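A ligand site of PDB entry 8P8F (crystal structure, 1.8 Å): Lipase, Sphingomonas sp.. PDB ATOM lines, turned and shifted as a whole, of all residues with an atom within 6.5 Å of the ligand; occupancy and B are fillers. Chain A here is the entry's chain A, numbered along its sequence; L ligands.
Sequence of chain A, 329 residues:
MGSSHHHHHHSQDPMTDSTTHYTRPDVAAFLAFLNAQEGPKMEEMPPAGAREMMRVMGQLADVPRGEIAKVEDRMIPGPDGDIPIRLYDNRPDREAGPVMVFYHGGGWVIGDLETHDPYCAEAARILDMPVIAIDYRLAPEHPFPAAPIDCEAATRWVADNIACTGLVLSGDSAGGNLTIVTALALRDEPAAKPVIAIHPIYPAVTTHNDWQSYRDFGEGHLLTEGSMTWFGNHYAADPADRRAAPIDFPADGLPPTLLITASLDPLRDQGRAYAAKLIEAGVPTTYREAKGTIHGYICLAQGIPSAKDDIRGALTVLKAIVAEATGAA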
ATOM      1  N   MET A  42     -28.564  13.138  13.876  1.00  0.00           N
ATOM      2  CA  MET A  42     -27.666  14.234  13.738  1.00  0.00           C
ATOM      3  C   MET A  42     -28.153  15.163  12.635  1.00  0.00           C
ATOM      4  O   MET A  42     -28.033  16.391  12.747  1.00  0.00           O
ATOM      5  CB  MET A  42     -26.278  13.696  13.372  1.00  0.00           C
ATOM      6  CG  MET A  42     -25.232  14.797  13.343  1.00  0.00           C
ATOM      7  SD  MET A  42     -23.747  14.244  12.513  1.00  0.00           S
ATOM      8  CE  MET A  42     -24.309  14.334  10.814  1.00  0.00           C
ATOM      9  N   MET A  54     -21.598  14.545  19.048  1.00  0.00           N
ATOM     10  CA  MET A  54     -20.373  13.791  18.903  1.00  0.00           C
ATOM     11  C   MET A  54     -19.560  13.859  20.202  1.00  0.00           C
ATOM     12  O   MET A  54     -18.910  12.898  20.572  1.00  0.00           O
ATOM     13  CB  MET A  54     -19.535  14.247  17.718  1.00  0.00           C
ATOM     14  CG  MET A  54     -18.318  13.308  17.453  1.00  0.00           C
ATOM     15  SD  MET A  54     -17.303  13.953  16.106  1.00  0.00           S
ATOM     16  CE  MET A  54     -16.882  12.449  15.237  1.00  0.00           C
ATOM     17  N   HIS A 104      -8.643  15.389  12.544  1.00  0.00           N
ATOM     18  CA  HIS A 104      -9.821  14.640  13.012  1.00  0.00           C
ATOM     19  C   HIS A 104     -10.904  14.604  11.921  1.00  0.00           C
ATOM     20  O   HIS A 104     -10.926  15.403  11.024  1.00  0.00           O
ATOM     21  CB  HIS A 104     -10.380  15.280  14.244  1.00  0.00           C
ATOM     22  CG  HIS A 104     -11.011  16.586  13.957  1.00  0.00           C
ATOM     23  ND1 HIS A 104     -12.379  16.675  13.731  1.00  0.00           N
ATOM     24  CD2 HIS A 104     -10.558  17.858  14.066  1.00  0.00           C
ATOM     25  CE1 HIS A 104     -12.672  17.967  13.491  1.00  0.00           C
ATOM     26  NE2 HIS A 104     -11.578  18.691  13.771  1.00  0.00           N
ATOM     27  N   GLY A 105     -11.803  13.630  12.050  1.00  0.00           N
ATOM     28  CA  GLY A 105     -12.933  13.508  11.168  1.00  0.00           C
ATOM     29  C   GLY A 105     -14.135  14.177  11.834  1.00  0.00           C
ATOM     30  O   GLY A 105     -14.009  14.724  12.924  1.00  0.00           O
ATOM     31  N   GLY A 106     -15.307  13.961  11.229  1.00  0.00           N
ATOM     32  CA  GLY A 106     -16.514  14.697  11.573  1.00  0.00           C
ATOM     33  C   GLY A 106     -17.133  15.370  10.361  1.00  0.00           C
ATOM     34  O   GLY A 106     -17.769  16.399  10.498  1.00  0.00           O
ATOM     35  N   GLY A 107     -16.902  14.821   9.178  1.00  0.00           N
ATOM     36  CA  GLY A 107     -17.473  15.265   7.888  1.00  0.00           C
ATOM     37  C   GLY A 107     -17.288  16.753   7.572  1.00  0.00           C
ATOM     38  O   GLY A 107     -18.105  17.327   6.864  1.00  0.00           O
ATOM     39  N   TRP A 108     -16.164  17.333   8.020  1.00  0.00           N
ATOM     40  CA  TRP A 108     -15.778  18.728   7.817  1.00  0.00           C
ATOM     41  C   TRP A 108     -16.721  19.715   8.508  1.00  0.00           C
ATOM     42  O   TRP A 108     -16.582  20.941   8.300  1.00  0.00           O
ATOM     43  CB  TRP A 108     -15.613  19.050   6.328  1.00  0.00           C
ATOM     44  CG  TRP A 108     -14.694  18.131   5.576  1.00  0.00           C
ATOM     45  CD1 TRP A 108     -13.327  18.185   5.451  1.00  0.00           C
ATOM     46  CD2 TRP A 108     -15.130  17.075   4.697  1.00  0.00           C
ATOM     47  NE1 TRP A 108     -12.878  17.155   4.674  1.00  0.00           N
ATOM     48  CE2 TRP A 108     -13.950  16.486   4.172  1.00  0.00           C
ATOM     49  CE3 TRP A 108     -16.358  16.545   4.344  1.00  0.00           C
ATOM     50  CZ2 TRP A 108     -14.002  15.383   3.310  1.00  0.00           C
ATOM     51  CZ3 TRP A 108     -16.399  15.432   3.556  1.00  0.00           C
ATOM     52  CH2 TRP A 108     -15.244  14.930   2.973  1.00  0.00           C
ATOM     53  N   ILE A 110     -18.223  18.672  12.117  1.00  0.00           N
ATOM     54  CA  ILE A 110     -18.158  18.384  13.550  1.00  0.00           C
ATOM     55  C   ILE A 110     -16.752  17.860  13.919  1.00  0.00           C
ATOM     56  O   ILE A 110     -15.899  17.785  13.048  1.00  0.00           O
ATOM     57  CB  ILE A 110     -19.287  17.449  13.991  1.00  0.00           C
ATOM     58  CG1 ILE A 110     -19.161  15.997  13.525  1.00  0.00           C
ATOM     59  CG2 ILE A 110     -20.627  18.018  13.549  1.00  0.00           C
ATOM     60  CD1 ILE A 110     -20.258  15.073  14.043  1.00  0.00           C
ATOM     61  N   HIS A 116     -11.335  13.565  19.512  1.00  0.00           N
ATOM     62  CA  HIS A 116     -10.342  12.581  19.099  1.00  0.00           C
ATOM     63  C   HIS A 116      -9.155  12.573  20.061  1.00  0.00           C
ATOM     64  O   HIS A 116      -8.096  11.991  19.766  1.00  0.00           O
ATOM     65  CB  HIS A 116      -9.846  12.905  17.687  1.00  0.00           C
ATOM     66  CG  HIS A 116     -10.922  12.636  16.662  1.00  0.00           C
ATOM     67  ND1 HIS A 116     -12.153  13.294  16.635  1.00  0.00           N
ATOM     68  CD2 HIS A 116     -10.988  11.734  15.675  1.00  0.00           C
ATOM     69  CE1 HIS A 116     -12.862  12.898  15.616  1.00  0.00           C
ATOM     70  NE2 HIS A 116     -12.182  11.934  14.985  1.00  0.00           N
ATOM     71  N   ASP A 172      -8.875  10.558  10.153  1.00  0.00           N
ATOM     72  CA  ASP A 172      -9.985   9.623  10.062  1.00  0.00           C
ATOM     73  C   ASP A 172     -11.160  10.221   9.295  1.00  0.00           C
ATOM     74  O   ASP A 172     -11.479  11.386   9.485  1.00  0.00           O
ATOM     75  CB  ASP A 172     -10.458   9.134  11.430  1.00  0.00           C
ATOM     76  CG  ASP A 172     -11.034  10.272  12.239  1.00  0.00           C
ATOM     77  OD1 ASP A 172     -10.243  11.168  12.513  1.00  0.00           O
ATOM     78  OD2 ASP A 172     -12.254  10.260  12.561  1.00  0.00           O
ATOM     79  N   SER A 173     -11.610   9.561   8.265  1.00  0.00           N
ATOM     80  CA  SER A 173     -12.828   9.964   7.493  1.00  0.00           C
ATOM     81  C   SER A 173     -12.571  11.271   6.723  1.00  0.00           C
ATOM     82  O   SER A 173     -11.656  11.287   5.882  1.00  0.00           O
ATOM     83  CB  SER A 173     -14.071   9.974   8.482  1.00  0.00           C
ATOM     84  OG  SER A 173     -15.306  10.520   7.972  1.00  0.00           O
ATOM     85  N   ALA A 174     -13.217  12.386   7.100  1.00  0.00           N
ATOM     86  CA  ALA A 174     -12.853  13.716   6.572  1.00  0.00           C
ATOM     87  C   ALA A 174     -11.359  14.009   6.736  1.00  0.00           C
ATOM     88  O   ALA A 174     -10.708  14.586   5.881  1.00  0.00           O
ATOM     89  CB  ALA A 174     -13.664  14.770   7.283  1.00  0.00           C
ATOM     90  N   GLY A 175     -10.848  13.646   7.930  1.00  0.00           N
ATOM     91  CA  GLY A 175      -9.426  13.783   8.228  1.00  0.00           C
ATOM     92  C   GLY A 175      -8.522  12.882   7.417  1.00  0.00           C
ATOM     93  O   GLY A 175      -7.347  13.116   7.276  1.00  0.00           O
ATOM     94  N   TYR A 202     -10.172   5.009   7.452  1.00  0.00           N
ATOM     95  CA  TYR A 202     -11.445   4.976   6.728  1.00  0.00           C
ATOM     96  C   TYR A 202     -11.724   6.279   6.008  1.00  0.00           C
ATOM     97  O   TYR A 202     -12.653   7.030   6.310  1.00  0.00           O
ATOM     98  CB  TYR A 202     -12.601   4.506   7.578  1.00  0.00           C
ATOM     99  CG  TYR A 202     -12.610   4.877   9.042  1.00  0.00           C
ATOM    100  CD1 TYR A 202     -12.944   6.145   9.429  1.00  0.00           C
ATOM    101  CD2 TYR A 202     -12.295   3.935  10.013  1.00  0.00           C
ATOM    102  CE1 TYR A 202     -13.067   6.475  10.770  1.00  0.00           C
ATOM    103  CE2 TYR A 202     -12.335   4.284  11.341  1.00  0.00           C
ATOM    104  CZ  TYR A 202     -12.738   5.549  11.711  1.00  0.00           C
ATOM    105  OH  TYR A 202     -12.772   5.886  13.046  1.00  0.00           O
ATOM    106  N   PRO A 203     -10.821   6.699   5.097  1.00  0.00           N
ATOM    107  CA  PRO A 203     -10.946   8.011   4.459  1.00  0.00           C
ATOM    108  C   PRO A 203     -12.082   8.135   3.418  1.00  0.00           C
ATOM    109  O   PRO A 203     -12.490   7.164   2.803  1.00  0.00           O
ATOM    110  CB  PRO A 203      -9.611   8.129   3.674  1.00  0.00           C
ATOM    111  CG  PRO A 203      -9.345   6.678   3.264  1.00  0.00           C
ATOM    112  CD  PRO A 203      -9.725   5.902   4.496  1.00  0.00           C
ATOM    113  N   ALA A 204     -12.547   9.386   3.235  1.00  0.00           N
ATOM    114  CA  ALA A 204     -13.279   9.805   2.043  1.00  0.00           C
ATOM    115  C   ALA A 204     -12.248  10.261   1.021  1.00  0.00           C
ATOM    116  O   ALA A 204     -11.307  10.971   1.395  1.00  0.00           O
ATOM    117  CB  ALA A 204     -14.255  10.903   2.375  1.00  0.00           C
ATOM    118  N   THR A 206     -13.596  10.818  -2.434  1.00  0.00           N
ATOM    119  CA  THR A 206     -14.405  11.329  -3.533  1.00  0.00           C
ATOM    120  C   THR A 206     -15.704  11.898  -2.995  1.00  0.00           C
ATOM    121  O   THR A 206     -16.020  11.626  -1.856  1.00  0.00           O
ATOM    122  CB  THR A 206     -14.685  10.296  -4.637  1.00  0.00           C
ATOM    123  OG1 THR A 206     -15.403  10.958  -5.683  1.00  0.00           O
ATOM    124  CG2 THR A 206     -15.474   9.094  -4.210  1.00  0.00           C
ATOM    125  N   LEU A 222     -24.151   3.446  11.750  1.00  0.00           N
ATOM    126  CA  LEU A 222     -23.708   4.694  12.361  1.00  0.00           C
ATOM    127  C   LEU A 222     -23.577   5.798  11.329  1.00  0.00           C
ATOM    128  O   LEU A 222     -24.276   6.804  11.455  1.00  0.00           O
ATOM    129  CB  LEU A 222     -22.433   4.487  13.200  1.00  0.00           C
ATOM    130  CG  LEU A 222     -21.865   5.716  13.932  1.00  0.00           C
ATOM    131  CD1 LEU A 222     -22.903   6.338  14.857  1.00  0.00           C
ATOM    132  CD2 LEU A 222     -20.633   5.330  14.733  1.00  0.00           C
ATOM    133  N   LEU A 223     -22.694   5.661  10.338  1.00  0.00           N
ATOM    134  CA  LEU A 223     -22.571   6.649   9.263  1.00  0.00           C
ATOM    135  C   LEU A 223     -23.636   6.352   8.229  1.00  0.00           C
ATOM    136  O   LEU A 223     -23.606   5.335   7.583  1.00  0.00           O
ATOM    137  CB  LEU A 223     -21.171   6.557   8.629  1.00  0.00           C
ATOM    138  CG  LEU A 223     -20.931   7.515   7.466  1.00  0.00           C
ATOM    139  CD1 LEU A 223     -21.038   8.993   7.912  1.00  0.00           C
ATOM    140  CD2 LEU A 223     -19.550   7.237   6.848  1.00  0.00           C
ATOM    141  N   SER A 227     -26.709  11.347   7.185  1.00  0.00           N
ATOM    142  CA  SER A 227     -25.592  12.038   7.767  1.00  0.00           C
ATOM    143  C   SER A 227     -24.653  12.540   6.665  1.00  0.00           C
ATOM    144  O   SER A 227     -24.221  13.705   6.671  1.00  0.00           O
ATOM    145  CB  SER A 227     -24.904  11.145   8.724  1.00  0.00           C
ATOM    146  OG  SER A 227     -25.686  11.110   9.895  1.00  0.00           O
ATOM    147  N   MET A 228     -24.331  11.663   5.758  1.00  0.00           N
ATOM    148  CA  MET A 228     -23.425  11.952   4.643  1.00  0.00           C
ATOM    149  C   MET A 228     -23.964  13.068   3.758  1.00  0.00           C
ATOM    150  O   MET A 228     -23.245  13.998   3.359  1.00  0.00           O
ATOM    151  CB  MET A 228     -23.146  10.710   3.784  1.00  0.00           C
ATOM    152  CG  MET A 228     -22.325   9.704   4.540  1.00  0.00           C
ATOM    153  SD  MET A 228     -22.019   8.160   3.609  1.00  0.00           S
ATOM    154  CE  MET A 228     -23.560   7.265   3.791  1.00  0.00           C
ATOM    155  N   PHE A 231     -23.571  16.416   5.908  1.00  0.00           N
ATOM    156  CA  PHE A 231     -22.177  16.851   5.888  1.00  0.00           C
ATOM    157  C   PHE A 231     -21.849  17.470   4.529  1.00  0.00           C
ATOM    158  O   PHE A 231     -21.265  18.565   4.456  1.00  0.00           O
ATOM    159  CB  PHE A 231     -21.201  15.707   6.142  1.00  0.00           C
ATOM    160  CG  PHE A 231     -21.173  15.092   7.505  1.00  0.00           C
ATOM    161  CD1 PHE A 231     -21.114  15.873   8.625  1.00  0.00           C
ATOM    162  CD2 PHE A 231     -21.073  13.699   7.653  1.00  0.00           C
ATOM    163  CE1 PHE A 231     -20.918  15.316   9.889  1.00  0.00           C
ATOM    164  CE2 PHE A 231     -20.976  13.133   8.929  1.00  0.00           C
ATOM    165  CZ  PHE A 231     -20.856  13.940  10.039  1.00  0.00           C
ATOM    166  N   LEU A 267     -17.996   4.039   3.239  1.00  0.00           N
ATOM    167  CA  LEU A 267     -16.762   4.501   2.612  1.00  0.00           C
ATOM    168  C   LEU A 267     -15.746   3.417   2.268  1.00  0.00           C
ATOM    169  O   LEU A 267     -14.665   3.751   1.687  1.00  0.00           O
ATOM    170  CB  LEU A 267     -16.088   5.531   3.506  1.00  0.00           C
ATOM    171  CG  LEU A 267     -16.888   6.775   3.897  1.00  0.00           C
ATOM    172  CD1 LEU A 267     -15.982   7.791   4.585  1.00  0.00           C
ATOM    173  CD2 LEU A 267     -17.609   7.390   2.754  1.00  0.00           C
ATOM    174  N   HIS A 295     -17.542   2.222  10.411  1.00  0.00           N
ATOM    175  CA  HIS A 295     -17.101   3.617  10.435  1.00  0.00           C
ATOM    176  C   HIS A 295     -17.078   4.210  11.854  1.00  0.00           C
ATOM    177  O   HIS A 295     -17.990   4.025  12.676  1.00  0.00           O
ATOM    178  CB  HIS A 295     -17.945   4.483   9.525  1.00  0.00           C
ATOM    179  CG  HIS A 295     -17.308   5.809   9.289  1.00  0.00           C
ATOM    180  ND1 HIS A 295     -16.412   5.946   8.235  1.00  0.00           N
ATOM    181  CD2 HIS A 295     -17.446   6.994   9.841  1.00  0.00           C
ATOM    182  CE1 HIS A 295     -16.020   7.197   8.179  1.00  0.00           C
ATOM    183  NE2 HIS A 295     -16.633   7.852   9.150  1.00  0.00           N
ATOM    184  N   GLY A 296     -15.917   4.822  12.176  1.00  0.00           N
ATOM    185  CA  GLY A 296     -15.777   5.647  13.381  1.00  0.00           C
ATOM    186  C   GLY A 296     -15.239   4.900  14.577  1.00  0.00           C
ATOM    187  O   GLY A 296     -15.212   5.508  15.617  1.00  0.00           O
ATOM    188  N   CYS A 299     -12.953   6.266  17.670  1.00  0.00           N
ATOM    189  CA  CYS A 299     -13.488   6.980  18.824  1.00  0.00           C
ATOM    190  C   CYS A 299     -14.553   6.202  19.608  1.00  0.00           C
ATOM    191  O   CYS A 299     -15.342   6.797  20.351  1.00  0.00           O
ATOM    192  CB  CYS A 299     -14.046   8.334  18.377  1.00  0.00           C
ATOM    193  SG  CYS A 299     -12.776   9.331  17.582  1.00  0.00           S
ATOM    194  N   LEU A 300     -14.540   4.860  19.508  1.00  0.00           N
ATOM    195  CA  LEU A 300     -15.614   4.076  20.120  1.00  0.00           C
ATOM    196  C   LEU A 300     -14.997   2.931  20.894  1.00  0.00           C
ATOM    197  O   LEU A 300     -15.555   1.866  20.978  1.00  0.00           O
ATOM    198  CB  LEU A 300     -16.570   3.552  19.030  1.00  0.00           C
ATOM    199  CG  LEU A 300     -17.396   4.602  18.317  1.00  0.00           C
ATOM    200  CD1 LEU A 300     -18.140   3.993  17.144  1.00  0.00           C
ATOM    201  CD2 LEU A 300     -18.309   5.271  19.323  1.00  0.00           C
HETATM  202  C1  LIG L   1     -18.752  10.770   5.261  1.00  0.00           C
HETATM  203  C2  LIG L   1     -18.269   9.255  13.630  1.00  0.00           C
HETATM  204  C3  LIG L   1     -19.609   9.533  13.441  1.00  0.00           C
HETATM  205  C4  LIG L   1     -19.995  10.277  12.340  1.00  0.00           C
HETATM  206  C5  LIG L   1     -19.050  10.741  11.431  1.00  0.00           C
HETATM  207  C6  LIG L   1     -18.120  11.421   4.237  1.00  0.00           C
HETATM  208  C7  LIG L   1     -18.224  10.807   6.568  1.00  0.00           C
HETATM  209  C8  LIG L   1     -16.429  11.560   8.225  1.00  0.00           C
HETATM  210  C9  LIG L   1     -16.994  12.131   4.566  1.00  0.00           C
HETATM  211  N1  LIG L   1     -16.430  12.168   5.816  1.00  0.00           N
HETATM  212  C10 LIG L   1     -17.040  11.502   6.814  1.00  0.00           C
HETATM  213  N2  LIG L   1     -17.068  10.886   9.192  1.00  0.00           N
HETATM  214  O1  LIG L   1     -15.616  12.443   8.531  1.00  0.00           O
HETATM  215  C11 LIG L   1     -16.645  10.940  10.603  1.00  0.00           C
HETATM  216  C12 LIG L   1     -17.698  10.456  11.600  1.00  0.00           C
HETATM  217  C13 LIG L   1     -17.328   9.700  12.710  1.00  0.00           C
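The backbone NH of Gly 106 lies within hydrogen-bond range of an oxygen (O1) of the ligand.
OG of Ser 173 is covalently linked to C8 of the ligand, 1.6 Å away.
N2 of the ligand sits at hydrogen-bond distance from NE2 of His 295, at 3.1 Å.
An oxygen (O1) of the ligand lies within hydrogen-bond range of the backbone NH (N) of Gly 107, 2.8 Å away.
The backbone NH of Ala 174 lies within hydrogen-bond range of an oxygen (O1) of the ligand, 2.8 Å away.
The side-chain carboxylate (OD1) of Asp 172 lies within hydrogen-bond range of the backbone NH (N) of Gly 105 (3.0 Å).
OG of Ser 173 sits at hydrogen-bond distance from NE2 of His 295, 3.2 Å away.
The backbone carbonyl oxygen of Ser 173 is in hydrogen-bond range of the backbone NH of Ala 204 (3.4 Å).
The backbone carbonyl oxygen of Tyr 202 lies close to the backbone NH of Ser 173 (3.4 Å).
The backbone NH of Gly 105 lies within hydrogen-bond range of a ring nitrogen (NE2) of His 116 (3.4 Å).
Residues that only touch the ligand: Met 54 (3.8 Å), Gly 105 (3.9 Å), Trp 108 (3.5 Å), Ala 204 (3.7 Å), Leu 223 (3.6 Å), Met 228 (3.8 Å) and Phe 231 (3.9 Å).
The nearest printed residue that does not touch the ligand is Leu 267 (4.1 Å).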
